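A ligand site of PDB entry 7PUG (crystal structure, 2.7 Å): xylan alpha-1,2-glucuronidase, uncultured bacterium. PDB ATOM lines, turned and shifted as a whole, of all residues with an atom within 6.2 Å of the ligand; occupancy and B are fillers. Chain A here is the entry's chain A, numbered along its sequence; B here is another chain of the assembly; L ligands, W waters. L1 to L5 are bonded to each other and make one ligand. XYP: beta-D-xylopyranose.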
ATOM      1  N   ASN A 178      14.689  14.768  19.533  1.00  0.00           N
ATOM      2  CA  ASN A 178      15.135  16.085  19.134  1.00  0.00           C
ATOM      3  C   ASN A 178      14.284  17.110  19.865  1.00  0.00           C
ATOM      4  O   ASN A 178      13.280  16.776  20.502  1.00  0.00           O
ATOM      5  CB  ASN A 178      15.071  16.245  17.611  1.00  0.00           C
ATOM      6  CG  ASN A 178      15.720  17.519  17.128  1.00  0.00           C
ATOM      7  OD1 ASN A 178      15.153  18.263  16.340  1.00  0.00           O
ATOM      8  ND2 ASN A 178      16.902  17.799  17.649  1.00  0.00           N
ATOM      9  N   ASP A 179      14.692  18.371  19.784  1.00  0.00           N
ATOM     10  CA  ASP A 179      14.048  19.424  20.550  1.00  0.00           C
ATOM     11  C   ASP A 179      13.988  19.055  22.035  1.00  0.00           C
ATOM     12  O   ASP A 179      13.071  19.455  22.757  1.00  0.00           O
ATOM     13  CB  ASP A 179      12.649  19.695  20.010  1.00  0.00           C
ATOM     14  CG  ASP A 179      12.655  20.097  18.562  1.00  0.00           C
ATOM     15  OD1 ASP A 179      13.718  20.552  18.077  1.00  0.00           O
ATOM     16  OD2 ASP A 179      11.596  19.984  17.902  1.00  0.00           O
ATOM     17  N   ALA A 181      15.427  19.725  24.884  1.00  0.00           N
ATOM     18  CA  ALA A 181      15.450  20.471  26.140  1.00  0.00           C
ATOM     19  C   ALA A 181      14.256  21.413  26.197  1.00  0.00           C
ATOM     20  O   ALA A 181      13.809  21.911  25.160  1.00  0.00           O
ATOM     21  CB  ALA A 181      16.727  21.280  26.325  1.00  0.00           C
ATOM     22  N   MET A 221      20.920  14.918  20.304  1.00  0.00           N
ATOM     23  CA  MET A 221      22.197  15.500  19.910  1.00  0.00           C
ATOM     24  C   MET A 221      22.320  17.002  20.198  1.00  0.00           C
ATOM     25  O   MET A 221      23.277  17.624  19.740  1.00  0.00           O
ATOM     26  CB  MET A 221      22.454  15.229  18.420  1.00  0.00           C
ATOM     27  CG  MET A 221      21.297  15.586  17.497  1.00  0.00           C
ATOM     28  SD  MET A 221      20.975  17.366  17.372  1.00  0.00           S
ATOM     29  CE  MET A 221      21.542  17.687  15.717  1.00  0.00           C
ATOM     30  N   TRP A 222      21.387  17.587  20.952  1.00  0.00           N
ATOM     31  CA  TRP A 222      21.505  19.003  21.295  1.00  0.00           C
ATOM     32  C   TRP A 222      22.714  19.265  22.187  1.00  0.00           C
ATOM     33  O   TRP A 222      23.568  20.107  21.859  1.00  0.00           O
ATOM     34  CB  TRP A 222      20.216  19.489  21.970  1.00  0.00           C
ATOM     35  CG  TRP A 222      19.232  20.104  21.014  1.00  0.00           C
ATOM     36  CD1 TRP A 222      19.230  19.970  19.660  1.00  0.00           C
ATOM     37  CD2 TRP A 222      18.114  20.945  21.338  1.00  0.00           C
ATOM     38  NE1 TRP A 222      18.177  20.675  19.120  1.00  0.00           N
ATOM     39  CE2 TRP A 222      17.488  21.291  20.119  1.00  0.00           C
ATOM     40  CE3 TRP A 222      17.587  21.446  22.536  1.00  0.00           C
ATOM     41  CZ2 TRP A 222      16.357  22.106  20.069  1.00  0.00           C
ATOM     42  CZ3 TRP A 222      16.465  22.260  22.481  1.00  0.00           C
ATOM     43  CH2 TRP A 222      15.865  22.583  21.254  1.00  0.00           C
ATOM     44  N   ASP A 223      22.810  18.566  23.317  1.00  0.00           N
ATOM     45  CA  ASP A 223      23.929  18.704  24.238  1.00  0.00           C
ATOM     46  C   ASP A 223      24.579  17.379  24.576  1.00  0.00           C
ATOM     47  O   ASP A 223      25.417  17.325  25.470  1.00  0.00           O
ATOM     48  CB  ASP A 223      23.514  19.347  25.553  1.00  0.00           C
ATOM     49  CG  ASP A 223      23.007  20.726  25.350  1.00  0.00           C
ATOM     50  OD1 ASP A 223      23.789  21.554  24.817  1.00  0.00           O
ATOM     51  OD2 ASP A 223      21.825  20.968  25.679  1.00  0.00           O
ATOM     52  N   GLN A 257      27.954  17.338  18.910  1.00  0.00           N
ATOM     53  CA  GLN A 257      28.578  17.908  20.092  1.00  0.00           C
ATOM     54  C   GLN A 257      30.009  17.444  20.264  1.00  0.00           C
ATOM     55  O   GLN A 257      30.775  18.092  20.981  1.00  0.00           O
ATOM     56  CB  GLN A 257      27.760  17.564  21.334  1.00  0.00           C
ATOM     57  CG  GLN A 257      26.546  18.432  21.478  1.00  0.00           C
ATOM     58  CD  GLN A 257      26.918  19.863  21.764  1.00  0.00           C
ATOM     59  OE1 GLN A 257      27.726  20.125  22.666  1.00  0.00           O
ATOM     60  NE2 GLN A 257      26.341  20.796  21.015  1.00  0.00           N
ATOM     61  N   ASP A 305      22.561  24.144  12.345  1.00  0.00           N
ATOM     62  CA  ASP A 305      21.580  23.811  11.323  1.00  0.00           C
ATOM     63  C   ASP A 305      21.676  24.769  10.133  1.00  0.00           C
ATOM     64  O   ASP A 305      20.662  25.144   9.546  1.00  0.00           O
ATOM     65  CB  ASP A 305      20.165  23.811  11.889  1.00  0.00           C
ATOM     66  CG  ASP A 305      19.345  22.627  11.405  1.00  0.00           C
ATOM     67  OD1 ASP A 305      19.855  21.768  10.632  1.00  0.00           O
ATOM     68  OD2 ASP A 305      18.159  22.542  11.808  1.00  0.00           O
ATOM     69  N   ASN A 383       9.239  20.466   7.727  1.00  0.00           N
ATOM     70  CA  ASN A 383       9.146  20.646   9.182  1.00  0.00           C
ATOM     71  C   ASN A 383       7.706  20.806   9.641  1.00  0.00           C
ATOM     72  O   ASN A 383       7.481  21.080  10.818  1.00  0.00           O
ATOM     73  CB  ASN A 383       9.958  21.827   9.712  1.00  0.00           C
ATOM     74  CG  ASN A 383      11.373  21.841   9.179  1.00  0.00           C
ATOM     75  OD1 ASN A 383      12.162  20.918   9.443  1.00  0.00           O
ATOM     76  ND2 ASN A 383      11.714  22.887   8.429  1.00  0.00           N
ATOM     77  N   TYR A 410       8.912  20.642  16.110  1.00  0.00           N
ATOM     78  CA  TYR A 410       9.835  21.421  15.302  1.00  0.00           C
ATOM     79  C   TYR A 410      10.227  22.702  16.010  1.00  0.00           C
ATOM     80  O   TYR A 410       9.381  23.389  16.603  1.00  0.00           O
ATOM     81  CB  TYR A 410       9.247  21.737  13.925  1.00  0.00           C
ATOM     82  CG  TYR A 410      10.201  22.555  13.077  1.00  0.00           C
ATOM     83  CD1 TYR A 410       9.887  23.860  12.691  1.00  0.00           C
ATOM     84  CD2 TYR A 410      11.423  22.041  12.686  1.00  0.00           C
ATOM     85  CE1 TYR A 410      10.755  24.604  11.939  1.00  0.00           C
ATOM     86  CE2 TYR A 410      12.297  22.789  11.942  1.00  0.00           C
ATOM     87  CZ  TYR A 410      11.966  24.051  11.561  1.00  0.00           C
ATOM     88  OH  TYR A 410      12.865  24.784  10.805  1.00  0.00           O
ATOM     89  N   VAL A 411      11.512  23.036  15.934  1.00  0.00           N
ATOM     90  CA  VAL A 411      12.043  24.285  16.491  1.00  0.00           C
ATOM     91  C   VAL A 411      12.560  25.134  15.338  1.00  0.00           C
ATOM     92  O   VAL A 411      13.552  24.788  14.681  1.00  0.00           O
ATOM     93  CB  VAL A 411      13.142  24.039  17.536  1.00  0.00           C
ATOM     94  CG1 VAL A 411      13.883  25.335  17.803  1.00  0.00           C
ATOM     95  CG2 VAL A 411      12.555  23.464  18.836  1.00  0.00           C
ATOM     96  N   GLY A 412      11.879  26.246  15.094  1.00  0.00           N
ATOM     97  CA  GLY A 412      12.265  27.115  14.012  1.00  0.00           C
ATOM     98  C   GLY A 412      11.079  27.947  13.562  1.00  0.00           C
ATOM     99  O   GLY A 412      10.213  28.305  14.360  1.00  0.00           O
ATOM    100  N   ALA A 413      11.063  28.229  12.250  1.00  0.00           N
ATOM    101  CA  ALA A 413      10.049  29.069  11.634  1.00  0.00           C
ATOM    102  C   ALA A 413       8.764  28.279  11.393  1.00  0.00           C
ATOM    103  O   ALA A 413       8.791  27.053  11.279  1.00  0.00           O
ATOM    104  CB  ALA A 413      10.566  29.644  10.317  1.00  0.00           C
ATOM    105  N   PRO A 414       7.614  28.957  11.354  1.00  0.00           N
ATOM    106  CA  PRO A 414       7.474  30.369  11.726  1.00  0.00           C
ATOM    107  C   PRO A 414       7.443  30.555  13.239  1.00  0.00           C
ATOM    108  O   PRO A 414       7.671  31.654  13.740  1.00  0.00           O
ATOM    109  CB  PRO A 414       6.148  30.749  11.098  1.00  0.00           C
ATOM    110  CG  PRO A 414       5.367  29.502  11.113  1.00  0.00           C
ATOM    111  CD  PRO A 414       6.341  28.366  10.936  1.00  0.00           C
ATOM    112  N   ARG A 415       7.167  29.483  13.967  1.00  0.00           N
ATOM    113  CA  ARG A 415       7.286  29.490  15.414  1.00  0.00           C
ATOM    114  C   ARG A 415       7.511  28.056  15.870  1.00  0.00           C
ATOM    115  O   ARG A 415       6.906  27.131  15.323  1.00  0.00           O
ATOM    116  CB  ARG A 415       6.048  30.093  16.076  1.00  0.00           C
ATOM    117  CG  ARG A 415       6.082  30.158  17.597  1.00  0.00           C
ATOM    118  CD  ARG A 415       4.906  30.950  18.129  1.00  0.00           C
ATOM    119  NE  ARG A 415       5.138  32.385  18.001  1.00  0.00           N
ATOM    120  CZ  ARG A 415       4.230  33.326  18.247  1.00  0.00           C
ATOM    121  NH1 ARG A 415       2.986  33.011  18.573  1.00  0.00           N
ATOM    122  NH2 ARG A 415       4.578  34.603  18.161  1.00  0.00           N
ATOM    123  N   TRP A 635       9.696  33.476  17.112  1.00  0.00           N
ATOM    124  CA  TRP A 635       9.669  32.065  16.741  1.00  0.00           C
ATOM    125  C   TRP A 635      10.211  31.143  17.812  1.00  0.00           C
ATOM    126  O   TRP A 635       9.924  29.942  17.780  1.00  0.00           O
ATOM    127  CB  TRP A 635      10.471  31.829  15.461  1.00  0.00           C
ATOM    128  CG  TRP A 635      11.951  32.080  15.625  1.00  0.00           C
ATOM    129  CD1 TRP A 635      12.601  33.239  15.390  1.00  0.00           C
ATOM    130  CD2 TRP A 635      12.950  31.125  16.043  1.00  0.00           C
ATOM    131  NE1 TRP A 635      13.947  33.092  15.635  1.00  0.00           N
ATOM    132  CE2 TRP A 635      14.190  31.801  16.039  1.00  0.00           C
ATOM    133  CE3 TRP A 635      12.915  29.783  16.419  1.00  0.00           C
ATOM    134  CZ2 TRP A 635      15.391  31.185  16.407  1.00  0.00           C
ATOM    135  CZ3 TRP A 635      14.110  29.164  16.779  1.00  0.00           C
ATOM    136  CH2 TRP A 635      15.333  29.870  16.775  1.00  0.00           C
ATOM    137  N   ASN A 636      11.025  31.654  18.741  1.00  0.00           N
ATOM    138  CA  ASN A 636      11.714  30.805  19.699  1.00  0.00           C
ATOM    139  C   ASN A 636      11.099  30.958  21.093  1.00  0.00           C
ATOM    140  O   ASN A 636      10.433  31.943  21.407  1.00  0.00           O
ATOM    141  CB  ASN A 636      13.206  31.153  19.758  1.00  0.00           C
ATOM    142  CG  ASN A 636      14.076  29.937  20.033  1.00  0.00           C
ATOM    143  OD1 ASN A 636      13.573  28.849  20.366  1.00  0.00           O
ATOM    144  ND2 ASN A 636      15.398  30.114  19.911  1.00  0.00           N
ATOM    145  N   TYR B 773      10.178  32.965   4.467  1.00  0.00           N
ATOM    146  CA  TYR B 773       9.509  33.421   5.682  1.00  0.00           C
ATOM    147  C   TYR B 773       8.331  34.347   5.407  1.00  0.00           C
ATOM    148  O   TYR B 773       7.526  34.583   6.321  1.00  0.00           O
ATOM    149  CB  TYR B 773      10.505  34.129   6.613  1.00  0.00           C
ATOM    150  CG  TYR B 773      11.697  33.287   6.959  1.00  0.00           C
ATOM    151  CD1 TYR B 773      12.929  33.551   6.403  1.00  0.00           C
ATOM    152  CD2 TYR B 773      11.592  32.218   7.826  1.00  0.00           C
ATOM    153  CE1 TYR B 773      14.032  32.781   6.700  1.00  0.00           C
ATOM    154  CE2 TYR B 773      12.679  31.442   8.138  1.00  0.00           C
ATOM    155  CZ  TYR B 773      13.910  31.733   7.570  1.00  0.00           C
ATOM    156  OH  TYR B 773      15.007  30.969   7.856  1.00  0.00           O
ATOM    157  N   TYR B 777       6.795  29.292   5.238  1.00  0.00           N
ATOM    158  CA  TYR B 777       6.606  28.762   6.587  1.00  0.00           C
ATOM    159  C   TYR B 777       5.284  29.181   7.211  1.00  0.00           C
ATOM    160  O   TYR B 777       4.655  28.332   7.880  1.00  0.00           O
ATOM    161  CB  TYR B 777       7.815  29.155   7.458  1.00  0.00           C
ATOM    162  CG  TYR B 777       8.925  28.148   7.229  1.00  0.00           C
ATOM    163  CD1 TYR B 777       8.784  26.831   7.658  1.00  0.00           C
ATOM    164  CD2 TYR B 777      10.070  28.487   6.529  1.00  0.00           C
ATOM    165  CE1 TYR B 777       9.762  25.890   7.428  1.00  0.00           C
ATOM    166  CE2 TYR B 777      11.057  27.545   6.294  1.00  0.00           C
ATOM    167  CZ  TYR B 777      10.896  26.246   6.742  1.00  0.00           C
ATOM    168  OH  TYR B 777      11.856  25.281   6.509  1.00  0.00           O
HETATM  169  O1  XYP L   1      20.546  24.048  26.260  1.00  0.00           O
HETATM  170  C1  XYP L   1      20.778  24.365  24.912  1.00  0.00           C
HETATM  171  C2  XYP L   1      21.979  23.609  24.332  1.00  0.00           C
HETATM  172  C3  XYP L   1      22.180  23.895  22.811  1.00  0.00           C
HETATM  173  C4  XYP L   1      20.815  23.823  22.088  1.00  0.00           C
HETATM  174  C5  XYP L   1      19.761  24.596  22.897  1.00  0.00           C
HETATM  175  O2  XYP L   1      23.148  23.983  25.031  1.00  0.00           O
HETATM  176  O3  XYP L   1      23.205  23.046  22.322  1.00  0.00           O
HETATM  177  O4  XYP L   1      21.006  24.435  20.832  1.00  0.00           O
HETATM  178  O5  XYP L   1      19.620  24.048  24.194  1.00  0.00           O
HETATM  179  C1  XYP L   2      19.935  24.315  19.868  1.00  0.00           C
HETATM  180  C2  XYP L   2      19.358  25.703  19.646  1.00  0.00           C
HETATM  181  C3  XYP L   2      18.283  25.716  18.559  1.00  0.00           C
HETATM  182  C4  XYP L   2      18.758  24.965  17.316  1.00  0.00           C
HETATM  183  C5  XYP L   2      19.383  23.632  17.768  1.00  0.00           C
HETATM  184  O2  XYP L   2      18.760  26.127  20.851  1.00  0.00           O
HETATM  185  O3  XYP L   2      17.996  27.043  18.170  1.00  0.00           O
HETATM  186  O4  XYP L   2      17.665  24.732  16.447  1.00  0.00           O
HETATM  187  O5  XYP L   2      20.441  23.804  18.677  1.00  0.00           O
HETATM  188  C1  XYP L   3      17.675  25.606  15.279  1.00  0.00           C
HETATM  189  C2  XYP L   3      16.698  25.004  14.233  1.00  0.00           C
HETATM  190  C3  XYP L   3      16.614  25.828  12.931  1.00  0.00           C
HETATM  191  C4  XYP L   3      16.299  27.291  13.274  1.00  0.00           C
HETATM  192  C5  XYP L   3      17.280  27.724  14.381  1.00  0.00           C
HETATM  193  O2  XYP L   3      17.033  23.654  13.981  1.00  0.00           O
HETATM  194  O3  XYP L   3      15.641  25.275  12.084  1.00  0.00           O
HETATM  195  O4  XYP L   3      16.433  28.141  12.159  1.00  0.00           O
HETATM  196  O5  XYP L   3      17.283  26.925  15.546  1.00  0.00           O
HETATM  197  C1  XYP L   4      15.645  29.332  12.388  1.00  0.00           C
HETATM  198  C2  XYP L   4      16.522  30.498  11.921  1.00  0.00           C
HETATM  199  C3  XYP L   4      15.833  31.879  12.019  1.00  0.00           C
HETATM  200  C4  XYP L   4      14.386  31.873  11.469  1.00  0.00           C
HETATM  201  C5  XYP L   4      13.753  30.615  12.066  1.00  0.00           C
HETATM  202  O2  XYP L   4      17.701  30.537  12.700  1.00  0.00           O
HETATM  203  O3  XYP L   4      16.582  32.865  11.346  1.00  0.00           O
HETATM  204  O4  XYP L   4      13.740  33.059  11.848  1.00  0.00           O
HETATM  205  O5  XYP L   4      14.427  29.423  11.696  1.00  0.00           O
HETATM  206  C1  XYP L   5      13.027  33.781  10.794  1.00  0.00           C
HETATM  207  C2  XYP L   5      11.616  33.872  11.396  1.00  0.00           C
HETATM  208  C3  XYP L   5      10.532  34.870  10.888  1.00  0.00           C
HETATM  209  C4  XYP L   5      11.308  36.155  10.623  1.00  0.00           C
HETATM  210  C5  XYP L   5      12.605  35.796   9.885  1.00  0.00           C
HETATM  211  O2  XYP L   5      11.003  32.583  11.388  1.00  0.00           O
HETATM  212  O3  XYP L   5       9.549  34.964  11.903  1.00  0.00           O
HETATM  213  O4  XYP L   5      10.530  36.986   9.815  1.00  0.00           O
HETATM  214  O5  XYP L   5      13.538  35.063  10.642  1.00  0.00           O
HETATM  215  O   HOH W   1      10.171  35.924  14.982  1.00  0.00           O
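The side-chain carboxylate (OD1) of Asp 223 sits at hydrogen-bond distance from an oxygen (O2) of XYP L1. OD2 of Asp 305 sits at hydrogen-bond distance from O2 of XYP L3, 2.7 Å away. O3 of XYP L1 sits at hydrogen-bond distance from O of Trp 222 (3.0 Å). O3 of XYP L3 lies within hydrogen-bond range of OH of Tyr 410 (3.1 Å). An oxygen (O3) of XYP L3 lies close to the backbone carbonyl oxygen (O) of Val 411 (3.4 Å).
The side-chain amide nitrogen (NE2) of Gln 257 lies within hydrogen-bond range of the backbone carbonyl oxygen (O) of Trp 222 (3.0 Å). The side-chain amide nitrogen (ND2) of Asn 178 sits close to the indole nitrogen (NE1) of Trp 222, 3.5 Å away. The side-chain hydroxyl (OH) of Tyr 410 lies within hydrogen-bond range of the side-chain amide nitrogen (ND2) of Asn 383 (3.3 Å). OD2 of Asp 179 is in hydrogen-bond range of N of Tyr 410.
Residues that only touch the ligand: Ala 413 (3.2 Å), Tyr 773 of chain B (3.6 Å), Trp 635 (3.7 Å) and Gly 412 (3.9 Å). Hydrophobic or aromatic side chains within 4 Å of the ligand: Trp 222, Tyr 410, Ala 413, Trp 635 and Tyr 773 of chain B. Nine residues have an atom within 4 Å of the ligand: Trp 222, Asp 223, Asp 305, Tyr 410, Val 411, Gly 412, Ala 413, Trp 635 and Tyr 773 of chain B. The nearest printed residue that does not touch the ligand is Gln 257 (4.1 Å).
Water W1 lies within hydrogen-bond range of the backbone NH of Trp 635 and an oxygen (O3) of XYP L5.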
